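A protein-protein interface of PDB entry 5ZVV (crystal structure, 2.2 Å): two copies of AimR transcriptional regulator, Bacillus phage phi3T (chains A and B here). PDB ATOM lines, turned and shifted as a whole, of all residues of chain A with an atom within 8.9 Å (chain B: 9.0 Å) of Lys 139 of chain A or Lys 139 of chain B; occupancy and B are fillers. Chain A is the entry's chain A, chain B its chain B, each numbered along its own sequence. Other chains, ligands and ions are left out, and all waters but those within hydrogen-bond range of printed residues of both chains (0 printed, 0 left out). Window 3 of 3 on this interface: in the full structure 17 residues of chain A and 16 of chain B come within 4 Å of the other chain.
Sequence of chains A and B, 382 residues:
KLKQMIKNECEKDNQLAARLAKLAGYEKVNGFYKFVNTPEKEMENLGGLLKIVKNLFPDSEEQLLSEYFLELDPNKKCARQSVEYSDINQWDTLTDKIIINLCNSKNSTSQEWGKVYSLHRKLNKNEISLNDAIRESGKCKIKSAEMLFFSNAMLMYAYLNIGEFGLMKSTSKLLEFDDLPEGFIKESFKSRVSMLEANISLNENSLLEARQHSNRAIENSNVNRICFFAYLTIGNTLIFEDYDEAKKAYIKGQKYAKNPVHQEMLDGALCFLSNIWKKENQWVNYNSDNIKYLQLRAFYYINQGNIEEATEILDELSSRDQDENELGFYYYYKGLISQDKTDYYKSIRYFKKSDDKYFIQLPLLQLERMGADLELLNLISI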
ATOM      1  N   LYS A 115      -0.989  -3.123 -20.594  1.00  0.00           N
ATOM      2  CA  LYS A 115      -0.093  -3.275 -21.734  1.00  0.00           C
ATOM      3  C   LYS A 115       0.325  -4.727 -21.917  1.00  0.00           C
ATOM      4  O   LYS A 115       0.399  -5.219 -23.050  1.00  0.00           O
ATOM      5  CB  LYS A 115       1.127  -2.369 -21.562  1.00  0.00           C
ATOM      6  CG  LYS A 115       0.814  -0.895 -21.785  1.00  0.00           C
ATOM      7  CD  LYS A 115       1.655   0.013 -20.898  1.00  0.00           C
ATOM      8  CE  LYS A 115       3.126  -0.037 -21.260  1.00  0.00           C
ATOM      9  NZ  LYS A 115       3.938   0.835 -20.365  1.00  0.00           N
ATOM     10  N   VAL A 116       0.589  -5.435 -20.815  1.00  0.00           N
ATOM     11  CA  VAL A 116       0.998  -6.833 -20.921  1.00  0.00           C
ATOM     12  C   VAL A 116      -0.152  -7.687 -21.439  1.00  0.00           C
ATOM     13  O   VAL A 116       0.027  -8.516 -22.338  1.00  0.00           O
ATOM     14  CB  VAL A 116       1.525  -7.348 -19.571  1.00  0.00           C
ATOM     15  CG1 VAL A 116       1.808  -8.840 -19.646  1.00  0.00           C
ATOM     16  CG2 VAL A 116       2.783  -6.594 -19.178  1.00  0.00           C
ATOM     17  N   LEU A 119      -0.623  -7.072 -25.084  1.00  0.00           N
ATOM     18  CA  LEU A 119       0.299  -7.890 -25.868  1.00  0.00           C
ATOM     19  C   LEU A 119      -0.172  -9.336 -25.938  1.00  0.00           C
ATOM     20  O   LEU A 119      -0.125  -9.961 -27.004  1.00  0.00           O
ATOM     21  CB  LEU A 119       1.707  -7.821 -25.276  1.00  0.00           C
ATOM     22  CG  LEU A 119       2.436  -6.478 -25.329  1.00  0.00           C
ATOM     23  CD1 LEU A 119       3.806  -6.604 -24.690  1.00  0.00           C
ATOM     24  CD2 LEU A 119       2.556  -5.992 -26.761  1.00  0.00           C
ATOM     25  N   ASN A 131       8.548 -12.116 -31.362  1.00  0.00           N
ATOM     26  CA  ASN A 131       9.689 -11.281 -31.013  1.00  0.00           C
ATOM     27  C   ASN A 131       9.270  -9.831 -30.807  1.00  0.00           C
ATOM     28  O   ASN A 131       9.832  -9.143 -29.948  1.00  0.00           O
ATOM     29  CB  ASN A 131      10.771 -11.384 -32.091  1.00  0.00           C
ATOM     30  CG  ASN A 131      11.425 -12.749 -32.126  1.00  0.00           C
ATOM     31  OD1 ASN A 131      10.877 -13.729 -31.618  1.00  0.00           O
ATOM     32  ND2 ASN A 131      12.610 -12.820 -32.724  1.00  0.00           N
ATOM     33  N   ASP A 132       8.292  -9.354 -31.585  1.00  0.00           N
ATOM     34  CA  ASP A 132       7.739  -8.024 -31.345  1.00  0.00           C
ATOM     35  C   ASP A 132       7.073  -7.948 -29.979  1.00  0.00           C
ATOM     36  O   ASP A 132       7.103  -6.901 -29.322  1.00  0.00           O
ATOM     37  CB  ASP A 132       6.740  -7.658 -32.442  1.00  0.00           C
ATOM     38  CG  ASP A 132       7.412  -7.263 -33.738  1.00  0.00           C
ATOM     39  OD1 ASP A 132       8.657  -7.189 -33.768  1.00  0.00           O
ATOM     40  OD2 ASP A 132       6.688  -7.021 -34.729  1.00  0.00           O
ATOM     41  N   ALA A 133       6.453  -9.047 -29.541  1.00  0.00           N
ATOM     42  CA  ALA A 133       5.880  -9.084 -28.200  1.00  0.00           C
ATOM     43  C   ALA A 133       6.965  -9.092 -27.134  1.00  0.00           C
ATOM     44  O   ALA A 133       6.775  -8.523 -26.054  1.00  0.00           O
ATOM     45  CB  ALA A 133       4.971 -10.304 -28.047  1.00  0.00           C
ATOM     46  N   ILE A 134       8.104  -9.726 -27.417  1.00  0.00           N
ATOM     47  CA  ILE A 134       9.214  -9.707 -26.470  1.00  0.00           C
ATOM     48  C   ILE A 134       9.797  -8.300 -26.356  1.00  0.00           C
ATOM     49  O   ILE A 134      10.068  -7.813 -25.251  1.00  0.00           O
ATOM     50  CB  ILE A 134      10.276 -10.741 -26.884  1.00  0.00           C
ATOM     51  CG1 ILE A 134       9.674 -12.150 -26.868  1.00  0.00           C
ATOM     52  CG2 ILE A 134      11.490 -10.663 -25.967  1.00  0.00           C
ATOM     53  CD1 ILE A 134      10.626 -13.232 -27.324  1.00  0.00           C
ATOM     54  N   ARG A 135       9.986  -7.622 -27.492  1.00  0.00           N
ATOM     55  CA  ARG A 135      10.523  -6.263 -27.468  1.00  0.00           C
ATOM     56  C   ARG A 135       9.554  -5.301 -26.793  1.00  0.00           C
ATOM     57  O   ARG A 135       9.944  -4.535 -25.903  1.00  0.00           O
ATOM     58  CB  ARG A 135      10.839  -5.793 -28.887  1.00  0.00           C
ATOM     59  CG  ARG A 135      11.876  -6.634 -29.600  1.00  0.00           C
ATOM     60  CD  ARG A 135      12.230  -6.052 -30.956  1.00  0.00           C
ATOM     61  NE  ARG A 135      12.824  -7.062 -31.827  1.00  0.00           N
ATOM     62  CZ  ARG A 135      12.160  -7.708 -32.778  1.00  0.00           C
ATOM     63  NH1 ARG A 135      10.878  -7.444 -32.991  1.00  0.00           N
ATOM     64  NH2 ARG A 135      12.776  -8.616 -33.522  1.00  0.00           N
ATOM     65  N   GLU A 136       8.286  -5.319 -27.215  1.00  0.00           N
ATOM     66  CA  GLU A 136       7.281  -4.461 -26.593  1.00  0.00           C
ATOM     67  C   GLU A 136       7.165  -4.740 -25.102  1.00  0.00           C
ATOM     68  O   GLU A 136       6.996  -3.813 -24.300  1.00  0.00           O
ATOM     69  CB  GLU A 136       5.931  -4.651 -27.283  1.00  0.00           C
ATOM     70  CG  GLU A 136       5.668  -3.655 -28.393  1.00  0.00           C
ATOM     71  CD  GLU A 136       5.602  -2.231 -27.880  1.00  0.00           C
ATOM     72  OE1 GLU A 136       4.868  -1.986 -26.899  1.00  0.00           O
ATOM     73  OE2 GLU A 136       6.295  -1.360 -28.445  1.00  0.00           O
ATOM     74  N   SER A 137       7.255  -6.013 -24.711  1.00  0.00           N
ATOM     75  CA  SER A 137       7.310  -6.345 -23.294  1.00  0.00           C
ATOM     76  C   SER A 137       8.517  -5.695 -22.632  1.00  0.00           C
ATOM     77  O   SER A 137       8.447  -5.272 -21.471  1.00  0.00           O
ATOM     78  CB  SER A 137       7.345  -7.862 -23.110  1.00  0.00           C
ATOM     79  OG  SER A 137       7.404  -8.209 -21.738  1.00  0.00           O
ATOM     80  N   GLY A 138       9.632  -5.598 -23.360  1.00  0.00           N
ATOM     81  CA  GLY A 138      10.796  -4.918 -22.820  1.00  0.00           C
ATOM     82  C   GLY A 138      10.603  -3.422 -22.669  1.00  0.00           C
ATOM     83  O   GLY A 138      11.155  -2.812 -21.749  1.00  0.00           O
ATOM     84  N   LYS A 139       9.822  -2.811 -23.561  1.00  0.00           N
ATOM     85  CA  LYS A 139       9.599  -1.372 -23.483  1.00  0.00           C
ATOM     86  C   LYS A 139       8.684  -0.982 -22.330  1.00  0.00           C
ATOM     87  O   LYS A 139       8.745   0.162 -21.870  1.00  0.00           O
ATOM     88  CB  LYS A 139       9.014  -0.863 -24.800  1.00  0.00           C
ATOM     89  CG  LYS A 139       9.865  -1.180 -26.017  1.00  0.00           C
ATOM     90  CD  LYS A 139      11.264  -0.604 -25.875  1.00  0.00           C
ATOM     91  CE  LYS A 139      12.070  -0.789 -27.155  1.00  0.00           C
ATOM     92  NZ  LYS A 139      12.178  -2.223 -27.550  1.00  0.00           N
ATOM     93  N   CYS A 140       7.851  -1.905 -21.845  1.00  0.00           N
ATOM     94  CA  CYS A 140       6.891  -1.588 -20.795  1.00  0.00           C
ATOM     95  C   CYS A 140       7.542  -1.288 -19.450  1.00  0.00           C
ATOM     96  O   CYS A 140       6.866  -0.738 -18.575  1.00  0.00           O
ATOM     97  CB  CYS A 140       5.893  -2.738 -20.628  1.00  0.00           C
ATOM     98  SG  CYS A 140       4.839  -3.056 -22.068  1.00  0.00           S
ATOM     99  N   LYS A 141       8.820  -1.626 -19.269  1.00  0.00           N
ATOM    100  CA  LYS A 141       9.511  -1.494 -17.985  1.00  0.00           C
ATOM    101  C   LYS A 141       8.691  -2.146 -16.871  1.00  0.00           C
ATOM    102  O   LYS A 141       8.263  -1.507 -15.908  1.00  0.00           O
ATOM    103  CB  LYS A 141       9.820  -0.027 -17.669  1.00  0.00           C
ATOM    104  CG  LYS A 141      10.705   0.655 -18.706  1.00  0.00           C
ATOM    105  CD  LYS A 141      10.839   2.150 -18.448  1.00  0.00           C
ATOM    106  CE  LYS A 141      11.679   2.434 -17.216  1.00  0.00           C
ATOM    107  NZ  LYS A 141      11.868   3.897 -16.994  1.00  0.00           N
ATOM    108  N   ILE A 142       8.472  -3.451 -17.038  1.00  0.00           N
ATOM    109  CA  ILE A 142       7.596  -4.203 -16.147  1.00  0.00           C
ATOM    110  C   ILE A 142       8.216  -4.275 -14.759  1.00  0.00           C
ATOM    111  O   ILE A 142       9.362  -4.712 -14.594  1.00  0.00           O
ATOM    112  CB  ILE A 142       7.334  -5.604 -16.720  1.00  0.00           C
ATOM    113  CG1 ILE A 142       6.675  -5.491 -18.098  1.00  0.00           C
ATOM    114  CG2 ILE A 142       6.481  -6.428 -15.765  1.00  0.00           C
ATOM    115  CD1 ILE A 142       6.577  -6.799 -18.840  1.00  0.00           C
ATOM    116  N   LYS A 143       7.455  -3.852 -13.753  1.00  0.00           N
ATOM    117  CA  LYS A 143       7.925  -3.785 -12.373  1.00  0.00           C
ATOM    118  C   LYS A 143       7.287  -4.820 -11.462  1.00  0.00           C
ATOM    119  O   LYS A 143       7.987  -5.443 -10.661  1.00  0.00           O
ATOM    120  CB  LYS A 143       7.658  -2.392 -11.789  1.00  0.00           C
ATOM    121  CG  LYS A 143       8.077  -1.231 -12.673  1.00  0.00           C
ATOM    122  CD  LYS A 143       9.581  -1.046 -12.689  1.00  0.00           C
ATOM    123  CE  LYS A 143       9.949   0.306 -13.279  1.00  0.00           C
ATOM    124  NZ  LYS A 143      11.415   0.563 -13.230  1.00  0.00           N
ATOM    125  N   GLU B 112      26.034   1.866 -33.549  1.00  0.00           N
ATOM    126  CA  GLU B 112      25.032   0.824 -33.743  1.00  0.00           C
ATOM    127  C   GLU B 112      25.686  -0.541 -33.936  1.00  0.00           C
ATOM    128  O   GLU B 112      25.300  -1.526 -33.292  1.00  0.00           O
ATOM    129  CB  GLU B 112      24.151   1.183 -34.935  1.00  0.00           C
ATOM    130  CG  GLU B 112      23.363   0.033 -35.509  1.00  0.00           C
ATOM    131  CD  GLU B 112      22.454   0.493 -36.619  1.00  0.00           C
ATOM    132  OE1 GLU B 112      21.877   1.589 -36.482  1.00  0.00           O
ATOM    133  OE2 GLU B 112      22.329  -0.223 -37.632  1.00  0.00           O
ATOM    134  N   LYS B 115      27.049  -1.804 -30.658  1.00  0.00           N
ATOM    135  CA  LYS B 115      26.010  -2.287 -29.753  1.00  0.00           C
ATOM    136  C   LYS B 115      25.510  -3.665 -30.172  1.00  0.00           C
ATOM    137  O   LYS B 115      25.375  -4.570 -29.335  1.00  0.00           O
ATOM    138  CB  LYS B 115      24.853  -1.288 -29.703  1.00  0.00           C
ATOM    139  CG  LYS B 115      25.171  -0.009 -28.949  1.00  0.00           C
ATOM    140  CD  LYS B 115      24.068   1.021 -29.132  1.00  0.00           C
ATOM    141  CE  LYS B 115      24.306   2.240 -28.257  1.00  0.00           C
ATOM    142  NZ  LYS B 115      24.156   1.925 -26.808  1.00  0.00           N
ATOM    143  N   VAL B 116      25.233  -3.845 -31.465  1.00  0.00           N
ATOM    144  CA  VAL B 116      24.730  -5.133 -31.943  1.00  0.00           C
ATOM    145  C   VAL B 116      25.758  -6.230 -31.693  1.00  0.00           C
ATOM    146  O   VAL B 116      25.440  -7.289 -31.137  1.00  0.00           O
ATOM    147  CB  VAL B 116      24.343  -5.043 -33.430  1.00  0.00           C
ATOM    148  CG1 VAL B 116      23.897  -6.405 -33.945  1.00  0.00           C
ATOM    149  CG2 VAL B 116      23.245  -4.014 -33.630  1.00  0.00           C
ATOM    150  N   LEU B 119      25.965  -7.169 -28.067  1.00  0.00           N
ATOM    151  CA  LEU B 119      24.928  -8.132 -27.706  1.00  0.00           C
ATOM    152  C   LEU B 119      25.272  -9.526 -28.212  1.00  0.00           C
ATOM    153  O   LEU B 119      25.075 -10.519 -27.503  1.00  0.00           O
ATOM    154  CB  LEU B 119      23.575  -7.684 -28.261  1.00  0.00           C
ATOM    155  CG  LEU B 119      22.891  -6.488 -27.604  1.00  0.00           C
ATOM    156  CD1 LEU B 119      21.561  -6.216 -28.280  1.00  0.00           C
ATOM    157  CD2 LEU B 119      22.693  -6.735 -26.119  1.00  0.00           C
ATOM    158  N   ASN B 131      15.904 -13.559 -24.803  1.00  0.00           N
ATOM    159  CA  ASN B 131      14.866 -12.534 -24.788  1.00  0.00           C
ATOM    160  C   ASN B 131      15.433 -11.180 -24.378  1.00  0.00           C
ATOM    161  O   ASN B 131      15.062 -10.147 -24.950  1.00  0.00           O
ATOM    162  CB  ASN B 131      13.728 -12.956 -23.859  1.00  0.00           C
ATOM    163  CG  ASN B 131      12.887 -14.078 -24.445  1.00  0.00           C
ATOM    164  OD1 ASN B 131      13.257 -14.690 -25.448  1.00  0.00           O
ATOM    165  ND2 ASN B 131      11.748 -14.351 -23.820  1.00  0.00           N
ATOM    166  N   ASP B 132      16.335 -11.165 -23.390  1.00  0.00           N
ATOM    167  CA  ASP B 132      17.041  -9.932 -23.052  1.00  0.00           C
ATOM    168  C   ASP B 132      17.742  -9.353 -24.273  1.00  0.00           C
ATOM    169  O   ASP B 132      17.722  -8.137 -24.493  1.00  0.00           O
ATOM    170  CB  ASP B 132      18.061 -10.183 -21.940  1.00  0.00           C
ATOM    171  CG  ASP B 132      17.420 -10.443 -20.591  1.00  0.00           C
ATOM    172  OD1 ASP B 132      16.181 -10.358 -20.486  1.00  0.00           O
ATOM    173  OD2 ASP B 132      18.165 -10.737 -19.632  1.00  0.00           O
ATOM    174  N   ALA B 133      18.367 -10.211 -25.081  1.00  0.00           N
ATOM    175  CA  ALA B 133      19.048  -9.735 -26.280  1.00  0.00           C
ATOM    176  C   ALA B 133      18.055  -9.192 -27.300  1.00  0.00           C
ATOM    177  O   ALA B 133      18.351  -8.220 -28.006  1.00  0.00           O
ATOM    178  CB  ALA B 133      19.881 -10.861 -26.890  1.00  0.00           C
ATOM    179  N   ILE B 134      16.872  -9.801 -27.389  1.00  0.00           N
ATOM    180  CA  ILE B 134      15.845  -9.303 -28.302  1.00  0.00           C
ATOM    181  C   ILE B 134      15.395  -7.907 -27.881  1.00  0.00           C
ATOM    182  O   ILE B 134      15.294  -6.988 -28.707  1.00  0.00           O
ATOM    183  CB  ILE B 134      14.665 -10.293 -28.368  1.00  0.00           C
ATOM    184  CG1 ILE B 134      15.122 -11.617 -28.983  1.00  0.00           C
ATOM    185  CG2 ILE B 134      13.509  -9.714 -29.162  1.00  0.00           C
ATOM    186  CD1 ILE B 134      14.030 -12.652 -29.094  1.00  0.00           C
ATOM    187  N   ARG B 135      15.152  -7.737 -26.586  1.00  0.00           N
ATOM    188  CA  ARG B 135      14.731  -6.447 -26.050  1.00  0.00           C
ATOM    189  C   ARG B 135      15.799  -5.374 -26.264  1.00  0.00           C
ATOM    190  O   ARG B 135      15.524  -4.322 -26.842  1.00  0.00           O
ATOM    191  CB  ARG B 135      14.399  -6.569 -24.562  1.00  0.00           C
ATOM    192  CG  ARG B 135      12.954  -6.945 -24.277  1.00  0.00           C
ATOM    193  CD  ARG B 135      12.863  -8.282 -23.559  1.00  0.00           C
ATOM    194  NE  ARG B 135      12.027  -8.205 -22.364  1.00  0.00           N
ATOM    195  CZ  ARG B 135      12.204  -8.953 -21.280  1.00  0.00           C
ATOM    196  NH1 ARG B 135      11.396  -8.815 -20.238  1.00  0.00           N
ATOM    197  NH2 ARG B 135      13.189  -9.841 -21.237  1.00  0.00           N
ATOM    198  N   GLU B 136      17.014  -5.645 -25.795  1.00  0.00           N
ATOM    199  CA  GLU B 136      18.121  -4.702 -25.933  1.00  0.00           C
ATOM    200  C   GLU B 136      18.381  -4.359 -27.394  1.00  0.00           C
ATOM    201  O   GLU B 136      18.688  -3.207 -27.721  1.00  0.00           O
ATOM    202  CB  GLU B 136      19.379  -5.270 -25.278  1.00  0.00           C
ATOM    203  CG  GLU B 136      19.413  -5.087 -23.774  1.00  0.00           C
ATOM    204  CD  GLU B 136      19.494  -3.626 -23.378  1.00  0.00           C
ATOM    205  OE1 GLU B 136      20.247  -2.875 -24.034  1.00  0.00           O
ATOM    206  OE2 GLU B 136      18.799  -3.226 -22.420  1.00  0.00           O
ATOM    207  N   SER B 137      18.257  -5.344 -28.287  1.00  0.00           N
ATOM    208  CA  SER B 137      18.307  -5.046 -29.715  1.00  0.00           C
ATOM    209  C   SER B 137      17.185  -4.097 -30.104  1.00  0.00           C
ATOM    210  O   SER B 137      17.358  -3.244 -30.982  1.00  0.00           O
ATOM    211  CB  SER B 137      18.222  -6.336 -30.530  1.00  0.00           C
ATOM    212  OG  SER B 137      16.935  -6.914 -30.426  1.00  0.00           O
ATOM    213  N   GLY B 138      16.025  -4.229 -29.456  1.00  0.00           N
ATOM    214  CA  GLY B 138      14.981  -3.236 -29.632  1.00  0.00           C
ATOM    215  C   GLY B 138      15.387  -1.857 -29.147  1.00  0.00           C
ATOM    216  O   GLY B 138      14.839  -0.850 -29.600  1.00  0.00           O
ATOM    217  N   LYS B 139      16.353  -1.788 -28.229  1.00  0.00           N
ATOM    218  CA  LYS B 139      16.832  -0.502 -27.729  1.00  0.00           C
ATOM    219  C   LYS B 139      18.031   0.048 -28.495  1.00  0.00           C
ATOM    220  O   LYS B 139      18.373   1.221 -28.308  1.00  0.00           O
ATOM    221  CB  LYS B 139      17.204  -0.604 -26.244  1.00  0.00           C
ATOM    222  CG  LYS B 139      16.030  -0.533 -25.278  1.00  0.00           C
ATOM    223  CD  LYS B 139      15.484  -1.912 -24.965  1.00  0.00           C
ATOM    224  CE  LYS B 139      14.365  -1.853 -23.940  1.00  0.00           C
ATOM    225  NZ  LYS B 139      13.846  -3.213 -23.627  1.00  0.00           N
ATOM    226  N   CYS B 140      18.671  -0.752 -29.352  1.00  0.00           N
ATOM    227  CA  CYS B 140      19.948  -0.364 -29.948  1.00  0.00           C
ATOM    228  C   CYS B 140      19.827   0.688 -31.044  1.00  0.00           C
ATOM    229  O   CYS B 140      20.862   1.080 -31.598  1.00  0.00           O
ATOM    230  CB  CYS B 140      20.663  -1.595 -30.509  1.00  0.00           C
ATOM    231  SG  CYS B 140      21.372  -2.673 -29.256  1.00  0.00           S
ATOM    232  N   LYS B 141      18.617   1.148 -31.371  1.00  0.00           N
ATOM    233  CA  LYS B 141      18.413   2.168 -32.403  1.00  0.00           C
ATOM    234  C   LYS B 141      18.986   1.711 -33.746  1.00  0.00           C
ATOM    235  O   LYS B 141      19.715   2.439 -34.422  1.00  0.00           O
ATOM    236  CB  LYS B 141      19.010   3.511 -31.972  1.00  0.00           C
ATOM    237  CG  LYS B 141      18.468   4.016 -30.642  1.00  0.00           C
ATOM    238  CD  LYS B 141      19.222   5.238 -30.138  1.00  0.00           C
ATOM    239  CE  LYS B 141      18.964   6.459 -31.003  1.00  0.00           C
ATOM    240  NZ  LYS B 141      19.539   7.693 -30.396  1.00  0.00           N
ATOM    241  N   ILE B 142      18.637   0.487 -34.133  1.00  0.00           N
ATOM    242  CA  ILE B 142      19.198  -0.145 -35.322  1.00  0.00           C
ATOM    243  C   ILE B 142      18.565   0.470 -36.564  1.00  0.00           C
ATOM    244  O   ILE B 142      17.355   0.343 -36.785  1.00  0.00           O
ATOM    245  CB  ILE B 142      18.988  -1.665 -35.288  1.00  0.00           C
ATOM    246  CG1 ILE B 142      19.624  -2.261 -34.030  1.00  0.00           C
ATOM    247  CG2 ILE B 142      19.565  -2.311 -36.535  1.00  0.00           C
ATOM    248  CD1 ILE B 142      19.362  -3.739 -33.853  1.00  0.00           C
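O of Gly 138 of chain A is in hydrogen-bond range of NZ of Lys 139 of chain B, 3.3 Å away.
NH2 of Arg 135 of chain B lies within salt-bridge range of OD1 of Asp 132 of chain B (3.1 Å).
Among the printed residues, merely in contact across the chains: Ile 134 of chain A with Arg 135 of chain B (3.2 Å), Gly 138 of chain A with Arg 135 of chain B (3.3 Å), Arg 135 of chain A with Ile 134 of chain B (3.5 Å), Ile 134 of chain A with Asn 131 of chain B (3.5 Å), Lys 139 of chain A with Gly 138 of chain B (3.6 Å), Asn 131 of chain A with Ile 134 of chain B (3.8 Å), Lys 139 of chain A with Lys 139 of chain B (3.9 Å) and Ile 134 of chain A with Ile 134 of chain B (3.9 Å).
Printed residues of chain B within 4 Å of Asn 131 of chain A: Ile 134. Of the printed residues of chain B, Arg 135 of chain A touches Ile 134 (3.5 Å). Of the printed residues of chain B, Lys 139 of chain A touches Gly 138 (3.6 Å) and Lys 139 (3.9 Å). Cys 140 of chain A touches none of the printed residues of chain B. Lys 115 of chain B touches none of the printed residues of chain A. Of the printed residues of chain A, Ile 134 of chain B touches Asn 131, Ile 134 and Arg 135. Printed residues of chain A within 4 Å of Arg 135 of chain B: Ile 134 (3.2 Å) and Gly 138 (3.3 Å). Lys 139 of chain B touches just these residues of chain A: Gly 138 (3.3 Å) and Lys 139 (3.9 Å). No residue of chain A comes within 4 Å of Cys 140 of chain B. Lys 141 of chain B touches none of the printed residues of chain A. The nearest printed residue of chain A that does not touch Asn 131 of chain B is Arg 135 of chain A (6.2 Å).
Of the 16 printed residues of chain A, 5 touch a printed residue of chain B. Of the 16 printed residues of chain B, 5 touch a printed residue of chain A. Hydrophobic or aromatic side chains of chain B that line the printed part of chain A: Ile 134. Among the printed residues, no Asp or Glu carboxylate lies within 4 Å of a Lys or Arg side-chain nitrogen of the other chain.
Asn 131 of chain A touches Ile 134 of chain B, and with the chains exchanged Ile 134 of chain A touches Asn 131 of chain B. Gly 138 of chain A touches Arg 135 of chain B, but with the chains exchanged Arg 135 of chain A does not touch Gly 138 of chain B (4.2 Å). Gly 138 of chain A touches Lys 139 of chain B, and with the chains exchanged Lys 139 of chain A touches Gly 138 of chain B. Lys 139 of chain A touches its own counterpart, Lys 139 of chain B.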
